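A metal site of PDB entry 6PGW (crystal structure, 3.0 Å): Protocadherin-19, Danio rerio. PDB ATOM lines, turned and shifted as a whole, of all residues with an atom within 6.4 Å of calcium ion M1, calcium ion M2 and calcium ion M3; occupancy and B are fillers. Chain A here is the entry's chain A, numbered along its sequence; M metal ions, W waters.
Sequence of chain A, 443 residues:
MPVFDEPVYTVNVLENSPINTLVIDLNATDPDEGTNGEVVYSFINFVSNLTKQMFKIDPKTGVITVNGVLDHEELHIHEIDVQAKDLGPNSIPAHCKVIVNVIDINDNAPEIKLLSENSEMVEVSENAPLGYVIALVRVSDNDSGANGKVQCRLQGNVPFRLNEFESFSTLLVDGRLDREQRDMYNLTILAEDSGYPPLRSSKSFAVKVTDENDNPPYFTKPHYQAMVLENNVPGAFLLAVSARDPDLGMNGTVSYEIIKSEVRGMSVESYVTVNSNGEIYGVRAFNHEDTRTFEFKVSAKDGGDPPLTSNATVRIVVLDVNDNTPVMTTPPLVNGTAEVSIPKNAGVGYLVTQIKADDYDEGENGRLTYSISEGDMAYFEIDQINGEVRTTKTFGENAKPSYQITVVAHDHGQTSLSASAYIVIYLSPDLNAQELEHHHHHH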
ATOM      1  N   GLU A  15     -16.639 -16.158  18.713  1.00  0.00           N
ATOM      2  CA  GLU A  15     -17.584 -17.280  18.630  1.00  0.00           C
ATOM      3  C   GLU A  15     -18.989 -16.919  19.149  1.00  0.00           C
ATOM      4  O   GLU A  15     -19.137 -16.236  20.125  1.00  0.00           O
ATOM      5  CB  GLU A  15     -16.981 -18.457  19.421  1.00  0.00           C
ATOM      6  CG  GLU A  15     -17.908 -19.583  19.788  1.00  0.00           C
ATOM      7  CD  GLU A  15     -17.141 -20.871  20.113  1.00  0.00           C
ATOM      8  OE1 GLU A  15     -16.198 -20.901  20.960  1.00  0.00           O
ATOM      9  OE2 GLU A  15     -17.479 -21.886  19.506  1.00  0.00           O
ATOM     10  N   ASN A  16     -20.003 -17.361  18.451  1.00  0.00           N
ATOM     11  CA  ASN A  16     -21.392 -17.089  18.812  1.00  0.00           C
ATOM     12  C   ASN A  16     -21.776 -15.609  18.907  1.00  0.00           C
ATOM     13  O   ASN A  16     -22.725 -15.275  19.558  1.00  0.00           O
ATOM     14  CB  ASN A  16     -21.766 -17.845  20.105  1.00  0.00           C
ATOM     15  CG  ASN A  16     -21.368 -19.303  20.064  1.00  0.00           C
ATOM     16  OD1 ASN A  16     -21.339 -19.933  18.987  1.00  0.00           O
ATOM     17  ND2 ASN A  16     -21.065 -19.866  21.212  1.00  0.00           N
ATOM     18  N   LEU A  70     -21.101 -18.512  14.513  1.00  0.00           N
ATOM     19  CA  LEU A  70     -19.721 -18.776  14.317  1.00  0.00           C
ATOM     20  C   LEU A  70     -19.288 -19.768  15.368  1.00  0.00           C
ATOM     21  O   LEU A  70     -18.988 -19.384  16.477  1.00  0.00           O
ATOM     22  CB  LEU A  70     -18.914 -17.464  14.407  1.00  0.00           C
ATOM     23  CG  LEU A  70     -19.175 -16.475  13.257  1.00  0.00           C
ATOM     24  CD1 LEU A  70     -18.714 -15.077  13.614  1.00  0.00           C
ATOM     25  CD2 LEU A  70     -18.501 -16.952  11.971  1.00  0.00           C
ATOM     26  N   ASP A  71     -19.270 -21.050  15.015  1.00  0.00           N
ATOM     27  CA  ASP A  71     -18.841 -22.119  15.941  1.00  0.00           C
ATOM     28  C   ASP A  71     -17.336 -22.520  15.822  1.00  0.00           C
ATOM     29  O   ASP A  71     -16.964 -23.288  14.963  1.00  0.00           O
ATOM     30  CB  ASP A  71     -19.734 -23.346  15.731  1.00  0.00           C
ATOM     31  CG  ASP A  71     -19.510 -24.431  16.773  1.00  0.00           C
ATOM     32  OD1 ASP A  71     -18.975 -24.120  17.870  1.00  0.00           O
ATOM     33  OD2 ASP A  71     -19.874 -25.611  16.515  1.00  0.00           O
ATOM     34  N   HIS A  72     -16.488 -22.054  16.753  1.00  0.00           N
ATOM     35  CA  HIS A  72     -15.065 -22.534  16.841  1.00  0.00           C
ATOM     36  C   HIS A  72     -14.840 -24.054  16.727  1.00  0.00           C
ATOM     37  O   HIS A  72     -13.787 -24.497  16.212  1.00  0.00           O
ATOM     38  CB  HIS A  72     -14.372 -22.047  18.137  1.00  0.00           C
ATOM     39  CG  HIS A  72     -12.896 -22.373  18.184  1.00  0.00           C
ATOM     40  ND1 HIS A  72     -11.932 -21.568  17.601  1.00  0.00           N
ATOM     41  CD2 HIS A  72     -12.225 -23.415  18.737  1.00  0.00           C
ATOM     42  CE1 HIS A  72     -10.738 -22.106  17.795  1.00  0.00           C
ATOM     43  NE2 HIS A  72     -10.890 -23.220  18.483  1.00  0.00           N
ATOM     44  N   GLU A  73     -15.762 -24.835  17.245  1.00  0.00           N
ATOM     45  CA  GLU A  73     -15.627 -26.280  17.202  1.00  0.00           C
ATOM     46  C   GLU A  73     -15.925 -26.800  15.770  1.00  0.00           C
ATOM     47  O   GLU A  73     -15.463 -27.876  15.384  1.00  0.00           O
ATOM     48  CB  GLU A  73     -16.522 -26.915  18.264  1.00  0.00           C
ATOM     49  CG  GLU A  73     -16.035 -26.676  19.701  1.00  0.00           C
ATOM     50  CD  GLU A  73     -16.294 -25.280  20.239  1.00  0.00           C
ATOM     51  OE1 GLU A  73     -15.353 -24.667  20.800  1.00  0.00           O
ATOM     52  OE2 GLU A  73     -17.457 -24.773  20.138  1.00  0.00           O
ATOM     53  N   GLU A  74     -16.644 -26.010  14.997  1.00  0.00           N
ATOM     54  CA  GLU A  74     -17.017 -26.340  13.620  1.00  0.00           C
ATOM     55  C   GLU A  74     -15.940 -25.774  12.703  1.00  0.00           C
ATOM     56  O   GLU A  74     -15.117 -26.522  12.182  1.00  0.00           O
ATOM     57  CB  GLU A  74     -18.391 -25.727  13.334  1.00  0.00           C
ATOM     58  CG  GLU A  74     -19.047 -25.959  11.984  1.00  0.00           C
ATOM     59  CD  GLU A  74     -20.279 -25.037  11.792  1.00  0.00           C
ATOM     60  OE1 GLU A  74     -20.172 -23.802  12.097  1.00  0.00           O
ATOM     61  OE2 GLU A  74     -21.364 -25.539  11.370  1.00  0.00           O
ATOM     62  N   ILE A 103     -12.546 -16.670  17.531  1.00  0.00           N
ATOM     63  CA  ILE A 103     -11.935 -16.815  18.810  1.00  0.00           C
ATOM     64  C   ILE A 103     -12.793 -17.728  19.650  1.00  0.00           C
ATOM     65  O   ILE A 103     -13.989 -17.493  19.798  1.00  0.00           O
ATOM     66  CB  ILE A 103     -11.762 -15.454  19.501  1.00  0.00           C
ATOM     67  CG1 ILE A 103     -10.484 -14.718  18.984  1.00  0.00           C
ATOM     68  CG2 ILE A 103     -11.609 -15.639  20.994  1.00  0.00           C
ATOM     69  CD1 ILE A 103     -10.249 -14.692  17.461  1.00  0.00           C
ATOM     70  N   ASP A 104     -12.164 -18.791  20.156  1.00  0.00           N
ATOM     71  CA  ASP A 104     -12.799 -19.814  21.026  1.00  0.00           C
ATOM     72  C   ASP A 104     -13.231 -19.222  22.335  1.00  0.00           C
ATOM     73  O   ASP A 104     -12.462 -18.549  22.985  1.00  0.00           O
ATOM     74  CB  ASP A 104     -11.811 -20.925  21.345  1.00  0.00           C
ATOM     75  CG  ASP A 104     -12.407 -21.996  22.201  1.00  0.00           C
ATOM     76  OD1 ASP A 104     -13.617 -22.294  22.041  1.00  0.00           O
ATOM     77  OD2 ASP A 104     -11.662 -22.562  23.023  1.00  0.00           O
ATOM     78  N   ILE A 105     -14.474 -19.508  22.733  1.00  0.00           N
ATOM     79  CA  ILE A 105     -14.961 -19.190  24.087  1.00  0.00           C
ATOM     80  C   ILE A 105     -15.497 -20.465  24.775  1.00  0.00           C
ATOM     81  O   ILE A 105     -15.629 -21.529  24.121  1.00  0.00           O
ATOM     82  CB  ILE A 105     -15.992 -18.020  24.055  1.00  0.00           C
ATOM     83  CG1 ILE A 105     -17.293 -18.441  23.404  1.00  0.00           C
ATOM     84  CG2 ILE A 105     -15.424 -16.821  23.301  1.00  0.00           C
ATOM     85  CD1 ILE A 105     -18.234 -17.299  23.182  1.00  0.00           C
ATOM     86  N   ASN A 106     -15.752 -20.373  26.090  1.00  0.00           N
ATOM     87  CA  ASN A 106     -16.011 -21.508  26.959  1.00  0.00           C
ATOM     88  C   ASN A 106     -17.527 -21.821  26.975  1.00  0.00           C
ATOM     89  O   ASN A 106     -18.233 -21.615  27.967  1.00  0.00           O
ATOM     90  CB  ASN A 106     -15.470 -21.215  28.372  1.00  0.00           C
ATOM     91  CG  ASN A 106     -15.322 -22.460  29.221  1.00  0.00           C
ATOM     92  OD1 ASN A 106     -15.234 -23.555  28.687  1.00  0.00           O
ATOM     93  ND2 ASN A 106     -15.277 -22.294  30.560  1.00  0.00           N
ATOM     94  N   ASP A 107     -18.013 -22.317  25.838  1.00  0.00           N
ATOM     95  CA  ASP A 107     -19.450 -22.585  25.638  1.00  0.00           C
ATOM     96  C   ASP A 107     -19.828 -24.095  25.712  1.00  0.00           C
ATOM     97  O   ASP A 107     -20.987 -24.417  25.781  1.00  0.00           O
ATOM     98  CB  ASP A 107     -19.979 -21.898  24.335  1.00  0.00           C
ATOM     99  CG  ASP A 107     -19.268 -22.366  23.047  1.00  0.00           C
ATOM    100  OD1 ASP A 107     -18.069 -22.843  23.082  1.00  0.00           O
ATOM    101  OD2 ASP A 107     -19.910 -22.218  21.963  1.00  0.00           O
ATOM    102  N   ASN A 108     -18.821 -24.980  25.760  1.00  0.00           N
ATOM    103  CA  ASN A 108     -18.986 -26.419  26.027  1.00  0.00           C
ATOM    104  C   ASN A 108     -18.375 -26.776  27.389  1.00  0.00           C
ATOM    105  O   ASN A 108     -17.165 -26.663  27.599  1.00  0.00           O
ATOM    106  CB  ASN A 108     -18.273 -27.245  24.934  1.00  0.00           C
ATOM    107  CG  ASN A 108     -18.808 -27.002  23.542  1.00  0.00           C
ATOM    108  OD1 ASN A 108     -19.687 -27.696  23.095  1.00  0.00           O
ATOM    109  ND2 ASN A 108     -18.215 -26.049  22.833  1.00  0.00           N
ATOM    110  N   ALA A 109     -19.195 -27.274  28.300  1.00  0.00           N
ATOM    111  CA  ALA A 109     -18.713 -27.746  29.597  1.00  0.00           C
ATOM    112  C   ALA A 109     -18.367 -29.221  29.499  1.00  0.00           C
ATOM    113  O   ALA A 109     -18.586 -29.817  28.474  1.00  0.00           O
ATOM    114  CB  ALA A 109     -19.789 -27.503  30.650  1.00  0.00           C
ATOM    115  N   PRO A 110     -17.794 -29.812  30.565  1.00  0.00           N
ATOM    116  CA  PRO A 110     -17.344 -31.181  30.430  1.00  0.00           C
ATOM    117  C   PRO A 110     -18.466 -32.230  30.188  1.00  0.00           C
ATOM    118  O   PRO A 110     -19.655 -32.001  30.480  1.00  0.00           O
ATOM    119  CB  PRO A 110     -16.642 -31.444  31.764  1.00  0.00           C
ATOM    120  CG  PRO A 110     -16.141 -30.115  32.171  1.00  0.00           C
ATOM    121  CD  PRO A 110     -17.235 -29.185  31.775  1.00  0.00           C
ATOM    122  N   ASP A 141     -14.166 -32.058  26.945  1.00  0.00           N
ATOM    123  CA  ASP A 141     -14.676 -30.689  26.729  1.00  0.00           C
ATOM    124  C   ASP A 141     -14.305 -30.376  25.302  1.00  0.00           C
ATOM    125  O   ASP A 141     -13.182 -30.661  24.873  1.00  0.00           O
ATOM    126  CB  ASP A 141     -14.007 -29.677  27.693  1.00  0.00           C
ATOM    127  CG  ASP A 141     -14.728 -28.329  27.741  1.00  0.00           C
ATOM    128  OD1 ASP A 141     -14.856 -27.657  26.692  1.00  0.00           O
ATOM    129  OD2 ASP A 141     -15.125 -27.943  28.835  1.00  0.00           O
ATOM    130  N   ASN A 142     -15.235 -29.855  24.535  1.00  0.00           N
ATOM    131  CA  ASN A 142     -15.063 -29.755  23.100  1.00  0.00           C
ATOM    132  C   ASN A 142     -14.406 -28.464  22.717  1.00  0.00           C
ATOM    133  O   ASN A 142     -14.120 -28.258  21.543  1.00  0.00           O
ATOM    134  CB  ASN A 142     -16.400 -29.926  22.393  1.00  0.00           C
ATOM    135  CG  ASN A 142     -16.943 -31.344  22.519  1.00  0.00           C
ATOM    136  OD1 ASN A 142     -16.729 -32.016  23.534  1.00  0.00           O
ATOM    137  ND2 ASN A 142     -17.617 -31.810  21.498  1.00  0.00           N
ATOM    138  N   ASP A 143     -14.135 -27.583  23.683  1.00  0.00           N
ATOM    139  CA  ASP A 143     -13.389 -26.348  23.397  1.00  0.00           C
ATOM    140  C   ASP A 143     -11.897 -26.628  23.300  1.00  0.00           C
ATOM    141  O   ASP A 143     -11.420 -27.753  23.528  1.00  0.00           O
ATOM    142  CB  ASP A 143     -13.633 -25.273  24.467  1.00  0.00           C
ATOM    143  CG  ASP A 143     -15.099 -24.966  24.691  1.00  0.00           C
ATOM    144  OD1 ASP A 143     -15.792 -24.627  23.701  1.00  0.00           O
ATOM    145  OD2 ASP A 143     -15.538 -25.041  25.877  1.00  0.00           O
ATOM    146  N   SER A 144     -11.164 -25.557  22.983  1.00  0.00           N
ATOM    147  CA  SER A 144      -9.706 -25.544  22.946  1.00  0.00           C
ATOM    148  C   SER A 144      -9.107 -24.818  24.129  1.00  0.00           C
ATOM    149  O   SER A 144      -9.762 -24.010  24.760  1.00  0.00           O
ATOM    150  CB  SER A 144      -9.261 -24.872  21.657  1.00  0.00           C
ATOM    151  OG  SER A 144     -10.032 -25.361  20.570  1.00  0.00           O
ATOM    152  N   ALA A 146      -7.284 -23.836  27.753  1.00  0.00           N
ATOM    153  CA  ALA A 146      -7.807 -23.907  29.126  1.00  0.00           C
ATOM    154  C   ALA A 146      -9.285 -24.279  29.155  1.00  0.00           C
ATOM    155  O   ALA A 146      -9.727 -25.007  30.034  1.00  0.00           O
ATOM    156  CB  ALA A 146      -7.615 -22.569  29.811  1.00  0.00           C
ATOM    157  N   ASN A 147     -10.036 -23.734  28.199  1.00  0.00           N
ATOM    158  CA  ASN A 147     -11.444 -24.007  28.060  1.00  0.00           C
ATOM    159  C   ASN A 147     -11.693 -25.456  27.710  1.00  0.00           C
ATOM    160  O   ASN A 147     -12.781 -25.987  27.975  1.00  0.00           O
ATOM    161  CB  ASN A 147     -12.054 -23.118  26.986  1.00  0.00           C
ATOM    162  CG  ASN A 147     -12.122 -21.676  27.411  1.00  0.00           C
ATOM    163  OD1 ASN A 147     -11.950 -21.365  28.571  1.00  0.00           O
ATOM    164  ND2 ASN A 147     -12.418 -20.803  26.482  1.00  0.00           N
ATOM    165  N   GLY A 148     -10.687 -26.103  27.123  1.00  0.00           N
ATOM    166  CA  GLY A 148     -10.720 -27.531  26.874  1.00  0.00           C
ATOM    167  C   GLY A 148     -10.216 -28.440  27.994  1.00  0.00           C
ATOM    168  O   GLY A 148     -10.622 -29.573  28.050  1.00  0.00           O
ATOM    169  N   LYS A 149      -9.296 -27.951  28.831  1.00  0.00           N
ATOM    170  CA  LYS A 149      -8.645 -28.816  29.862  1.00  0.00           C
ATOM    171  C   LYS A 149      -9.544 -29.164  31.023  1.00  0.00           C
ATOM    172  O   LYS A 149     -10.287 -28.318  31.529  1.00  0.00           O
ATOM    173  CB  LYS A 149      -7.387 -28.143  30.426  1.00  0.00           C
ATOM    174  CG  LYS A 149      -6.130 -28.442  29.635  1.00  0.00           C
ATOM    175  CD  LYS A 149      -5.266 -27.182  29.497  1.00  0.00           C
ATOM    176  CE  LYS A 149      -4.231 -27.286  28.378  1.00  0.00           C
ATOM    177  NZ  LYS A 149      -3.662 -25.951  28.045  1.00  0.00           N
ATOM    178  N   VAL A 150      -9.447 -30.403  31.495  1.00  0.00           N
ATOM    179  CA  VAL A 150     -10.345 -30.865  32.557  1.00  0.00           C
ATOM    180  C   VAL A 150      -9.736 -31.866  33.553  1.00  0.00           C
ATOM    181  O   VAL A 150      -8.976 -32.768  33.175  1.00  0.00           O
ATOM    182  CB  VAL A 150     -11.607 -31.488  31.941  1.00  0.00           C
ATOM    183  CG1 VAL A 150     -12.197 -30.580  30.855  1.00  0.00           C
ATOM    184  CG2 VAL A 150     -11.296 -32.851  31.343  1.00  0.00           C
ATOM    185  N   ASP A 193     -14.093 -27.778  33.786  1.00  0.00           N
ATOM    186  CA  ASP A 193     -13.065 -27.330  32.806  1.00  0.00           C
ATOM    187  C   ASP A 193     -12.190 -26.271  33.398  1.00  0.00           C
ATOM    188  O   ASP A 193     -12.419 -25.853  34.489  1.00  0.00           O
ATOM    189  CB  ASP A 193     -13.662 -26.948  31.409  1.00  0.00           C
ATOM    190  CG  ASP A 193     -14.573 -25.690  31.410  1.00  0.00           C
ATOM    191  OD1 ASP A 193     -14.503 -24.853  32.335  1.00  0.00           O
ATOM    192  OD2 ASP A 193     -15.334 -25.543  30.403  1.00  0.00           O
ATOM    193  N   SER A 194     -11.134 -25.879  32.709  1.00  0.00           N
ATOM    194  CA  SER A 194     -10.191 -24.913  33.263  1.00  0.00           C
ATOM    195  C   SER A 194     -10.329 -23.509  32.693  1.00  0.00           C
ATOM    196  O   SER A 194      -9.386 -22.715  32.750  1.00  0.00           O
ATOM    197  CB  SER A 194      -8.757 -25.423  33.106  1.00  0.00           C
ATOM    198  OG  SER A 194      -8.694 -26.816  33.438  1.00  0.00           O
ATOM    199  N   GLY A 195     -11.524 -23.184  32.173  1.00  0.00           N
ATOM    200  CA  GLY A 195     -11.853 -21.804  31.773  1.00  0.00           C
ATOM    201  C   GLY A 195     -12.046 -20.880  32.977  1.00  0.00           C
ATOM    202  O   GLY A 195     -11.941 -21.319  34.107  1.00  0.00           O
ATOM    203  N   LEU A 199     -16.237 -24.126  34.047  1.00  0.00           N
ATOM    204  CA  LEU A 199     -17.571 -24.725  33.950  1.00  0.00           C
ATOM    205  C   LEU A 199     -17.534 -26.112  34.464  1.00  0.00           C
ATOM    206  O   LEU A 199     -16.632 -26.860  34.109  1.00  0.00           O
ATOM    207  CB  LEU A 199     -18.053 -24.725  32.506  1.00  0.00           C
ATOM    208  CG  LEU A 199     -18.779 -23.442  32.139  1.00  0.00           C
ATOM    209  CD1 LEU A 199     -18.656 -23.135  30.658  1.00  0.00           C
ATOM    210  CD2 LEU A 199     -20.237 -23.547  32.533  1.00  0.00           C
HETATM  211 CA    CA M   1     -15.098 -25.769  28.050  1.00  0.00          CA
HETATM  212 CA    CA M   2     -15.873 -22.865  22.221  1.00  0.00          CA
HETATM  213 CA    CA M   3     -19.207 -23.253  19.993  1.00  0.00          CA
HETATM  214  O   HOH W   1     -20.361 -25.279  19.999  1.00  0.00           O
HETATM  215  O   HOH W   2     -21.362 -22.725  19.316  1.00  0.00           O
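The backbone NH (N) of Glu 15 is in hydrogen-bond range of the backbone carbonyl oxygen (O) of Ile 103, 3.2 Å away.
The side-chain amide nitrogen of Asn 108 lies close to the side-chain carboxylate of Asp 107.
The side-chain carboxylate of Asp 193 sits at hydrogen-bond distance from the backbone NH of Leu 199.
The side-chain carboxylate (OD1) of Asp 193 sits close to the backbone NH (N) of Gly 195.
The side-chain carboxylate (OE2) of Glu 15 sits close to the backbone NH (N) of His 72 (2.9 Å).
OD2 of Asp 107 sits close to ND2 of Asn 16, at 2.7 Å.
The side-chain amide nitrogen of Asn 108 sits close to the side-chain carboxylate of Glu 73 (3.1 Å).
The side-chain carboxylate (OD2) of Asp 104 lies within hydrogen-bond range of the backbone NH (N) of Ser 144.
Within 4 Å of calcium ion M1: Asn 106, Asn 108, Asp 141, Asp 143, Asn 147 and Asp 193.
Of the 28 residues printed, 7 come within 4 Å of calcium ion M2.
Calcium ion M1 is bound by the backbone carbonyl oxygen (O) of Asn 108 (2.3 Å), the side-chain amide oxygen (OD1) of Asn 106 (2.3 Å), the side-chain carboxylate (OD2) of Asp 141 (2.3 Å), the backbone carbonyl oxygen (O) of Asn 147 (2.3 Å), the side-chain carboxylate (OD2) of Asp 143 (2.3 Å), the side-chain carboxylate (OD1) of Asp 141 (2.3 Å) and the side-chain carboxylate (OD2) of Asp 193 (2.4 Å).
Calcium ion M1 has seven donor atoms within binding distance.
Calcium ion M2 is bound by the side-chain carboxylate of Asp 143, the side-chain carboxylate of Asp 104, the backbone carbonyl oxygen of Ile 105, the side-chain carboxylate of Glu 73, the side-chain carboxylate of Glu 15 and the side-chain carboxylate of Asp 107.
Calcium ion M2 has six donor atoms within binding distance.
Calcium ion M3 is bound by OE2 of Glu 15 (2.3 Å), OD1 of Asp 71 (2.3 Å), water W2 (2.3 Å), OE2 of Glu 73 (2.3 Å), water W1 (2.3 Å) and OD2 of Asp 107 (2.3 Å).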
